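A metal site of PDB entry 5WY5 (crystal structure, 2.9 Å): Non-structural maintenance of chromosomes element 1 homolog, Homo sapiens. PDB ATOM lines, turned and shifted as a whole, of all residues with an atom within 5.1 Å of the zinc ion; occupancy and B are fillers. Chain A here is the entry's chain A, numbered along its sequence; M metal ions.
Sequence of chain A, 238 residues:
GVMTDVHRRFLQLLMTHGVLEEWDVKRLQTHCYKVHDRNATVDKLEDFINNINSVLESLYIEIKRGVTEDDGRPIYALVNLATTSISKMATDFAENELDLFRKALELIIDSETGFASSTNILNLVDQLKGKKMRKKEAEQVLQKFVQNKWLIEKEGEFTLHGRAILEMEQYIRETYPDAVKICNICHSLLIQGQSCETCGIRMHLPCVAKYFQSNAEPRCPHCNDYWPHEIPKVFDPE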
ATOM      1  N   CYS A 196      -4.412 -12.272   3.720  1.00  0.00           N
ATOM      2  CA  CYS A 196      -5.840 -12.338   4.035  1.00  0.00           C
ATOM      3  C   CYS A 196      -6.628 -11.962   2.801  1.00  0.00           C
ATOM      4  O   CYS A 196      -6.186 -11.119   2.013  1.00  0.00           O
ATOM      5  CB  CYS A 196      -6.204 -11.436   5.218  1.00  0.00           C
ATOM      6  SG  CYS A 196      -7.950 -11.609   5.781  1.00  0.00           S
ATOM      7  N   THR A 198      -9.588 -10.548   2.858  1.00  0.00           N
ATOM      8  CA  THR A 198     -10.354  -9.333   3.092  1.00  0.00           C
ATOM      9  C   THR A 198      -9.417  -8.127   3.215  1.00  0.00           C
ATOM     10  O   THR A 198      -9.558  -7.149   2.497  1.00  0.00           O
ATOM     11  CB  THR A 198     -11.261  -9.481   4.325  1.00  0.00           C
ATOM     12  OG1 THR A 198     -11.905 -10.753   4.273  1.00  0.00           O
ATOM     13  CG2 THR A 198     -12.318  -8.384   4.330  1.00  0.00           C
ATOM     14  N   CYS A 199      -8.447  -8.206   4.124  1.00  0.00           N
ATOM     15  CA  CYS A 199      -7.369  -7.250   4.100  1.00  0.00           C
ATOM     16  C   CYS A 199      -6.645  -7.456   2.807  1.00  0.00           C
ATOM     17  O   CYS A 199      -7.214  -7.856   1.798  1.00  0.00           O
ATOM     18  CB  CYS A 199      -6.367  -7.555   5.214  1.00  0.00           C
ATOM     19  SG  CYS A 199      -6.865  -7.179   6.895  1.00  0.00           S
ATOM     20  N   ILE A 201      -3.490  -8.204   4.062  1.00  0.00           N
ATOM     21  CA  ILE A 201      -2.455  -8.395   5.058  1.00  0.00           C
ATOM     22  C   ILE A 201      -1.705  -9.685   4.809  1.00  0.00           C
ATOM     23  O   ILE A 201      -2.286 -10.659   4.325  1.00  0.00           O
ATOM     24  CB  ILE A 201      -3.005  -8.325   6.501  1.00  0.00           C
ATOM     25  CG1 ILE A 201      -2.562  -7.023   7.158  1.00  0.00           C
ATOM     26  CG2 ILE A 201      -2.496  -9.469   7.362  1.00  0.00           C
ATOM     27  CD1 ILE A 201      -3.102  -5.780   6.466  1.00  0.00           C
ATOM     28  N   CYS A 220      -8.071 -13.115  11.506  1.00  0.00           N
ATOM     29  CA  CYS A 220      -7.134 -12.133  10.954  1.00  0.00           C
ATOM     30  C   CYS A 220      -6.952 -10.960  11.883  1.00  0.00           C
ATOM     31  O   CYS A 220      -7.898 -10.234  12.169  1.00  0.00           O
ATOM     32  CB  CYS A 220      -7.659 -11.640   9.611  1.00  0.00           C
ATOM     33  SG  CYS A 220      -6.811 -10.220   8.942  1.00  0.00           S
ATOM     34  N   HIS A 222      -5.583  -7.900  11.818  1.00  0.00           N
ATOM     35  CA  HIS A 222      -6.106  -6.650  11.271  1.00  0.00           C
ATOM     36  C   HIS A 222      -7.380  -7.028  10.532  1.00  0.00           C
ATOM     37  O   HIS A 222      -7.321  -7.791   9.584  1.00  0.00           O
ATOM     38  CB  HIS A 222      -5.101  -6.067  10.279  1.00  0.00           C
ATOM     39  CG  HIS A 222      -5.458  -4.689   9.778  1.00  0.00           C
ATOM     40  ND1 HIS A 222      -5.166  -3.541  10.483  1.00  0.00           N
ATOM     41  CD2 HIS A 222      -6.065  -4.288   8.636  1.00  0.00           C
ATOM     42  CE1 HIS A 222      -5.575  -2.491   9.794  1.00  0.00           C
ATOM     43  NE2 HIS A 222      -6.127  -2.912   8.674  1.00  0.00           N
ATOM     44  N   CYS A 223      -8.527  -6.525  10.991  1.00  0.00           N
ATOM     45  CA  CYS A 223      -9.826  -6.795  10.354  1.00  0.00           C
ATOM     46  C   CYS A 223     -10.585  -7.965  10.947  1.00  0.00           C
ATOM     47  O   CYS A 223     -11.773  -8.152  10.686  1.00  0.00           O
ATOM     48  CB  CYS A 223      -9.709  -6.999   8.839  1.00  0.00           C
ATOM     49  SG  CYS A 223      -9.689  -8.747   8.309  1.00  0.00           S
ATOM     50  N   ASP A 225     -11.387 -10.839  10.415  1.00  0.00           N
ATOM     51  CA  ASP A 225     -12.125 -11.825   9.630  1.00  0.00           C
ATOM     52  C   ASP A 225     -11.529 -13.203   9.863  1.00  0.00           C
ATOM     53  O   ASP A 225     -10.362 -13.334  10.239  1.00  0.00           O
ATOM     54  CB  ASP A 225     -12.063 -11.462   8.141  1.00  0.00           C
ATOM     55  CG  ASP A 225     -13.273 -11.965   7.366  1.00  0.00           C
ATOM     56  OD1 ASP A 225     -14.273 -12.377   7.999  1.00  0.00           O
ATOM     57  OD2 ASP A 225     -13.230 -11.937   6.116  1.00  0.00           O
HETATM   58 ZN    ZN M   1      -7.686  -9.357   6.947  1.00  0.00          ZN
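Merely in contact with the zinc ion: His 222 (3.1 Å). Of the 8 residues printed, 5 come within 4 Å of the zinc ion.
The side-chain sulfur (SG) of Cys 220 sits close to the backbone carbonyl oxygen (O) of His 222 (2.6 Å). SG of Cys 199 sits close to O of His 222. N of Thr 198 lies close to SG of Cys 196 (3.5 Å). SG of Cys 223 sits close to N of Asp 225, at 3.4 Å. O of Ile 201 lies within hydrogen-bond range of N of Cys 196, at 2.7 Å. N of Cys 220 lies within hydrogen-bond range of O of Asp 225, at 2.6 Å.
SG of Cys 199 is bound to the zinc ion, 2.3 Å away. SG of Cys 220 is bound to the zinc ion, 2.3 Å away. SG of Cys 223 is bound to the zinc ion, 2.5 Å away. The zinc ion is bound by SG of Cys 196 (2.5 Å).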
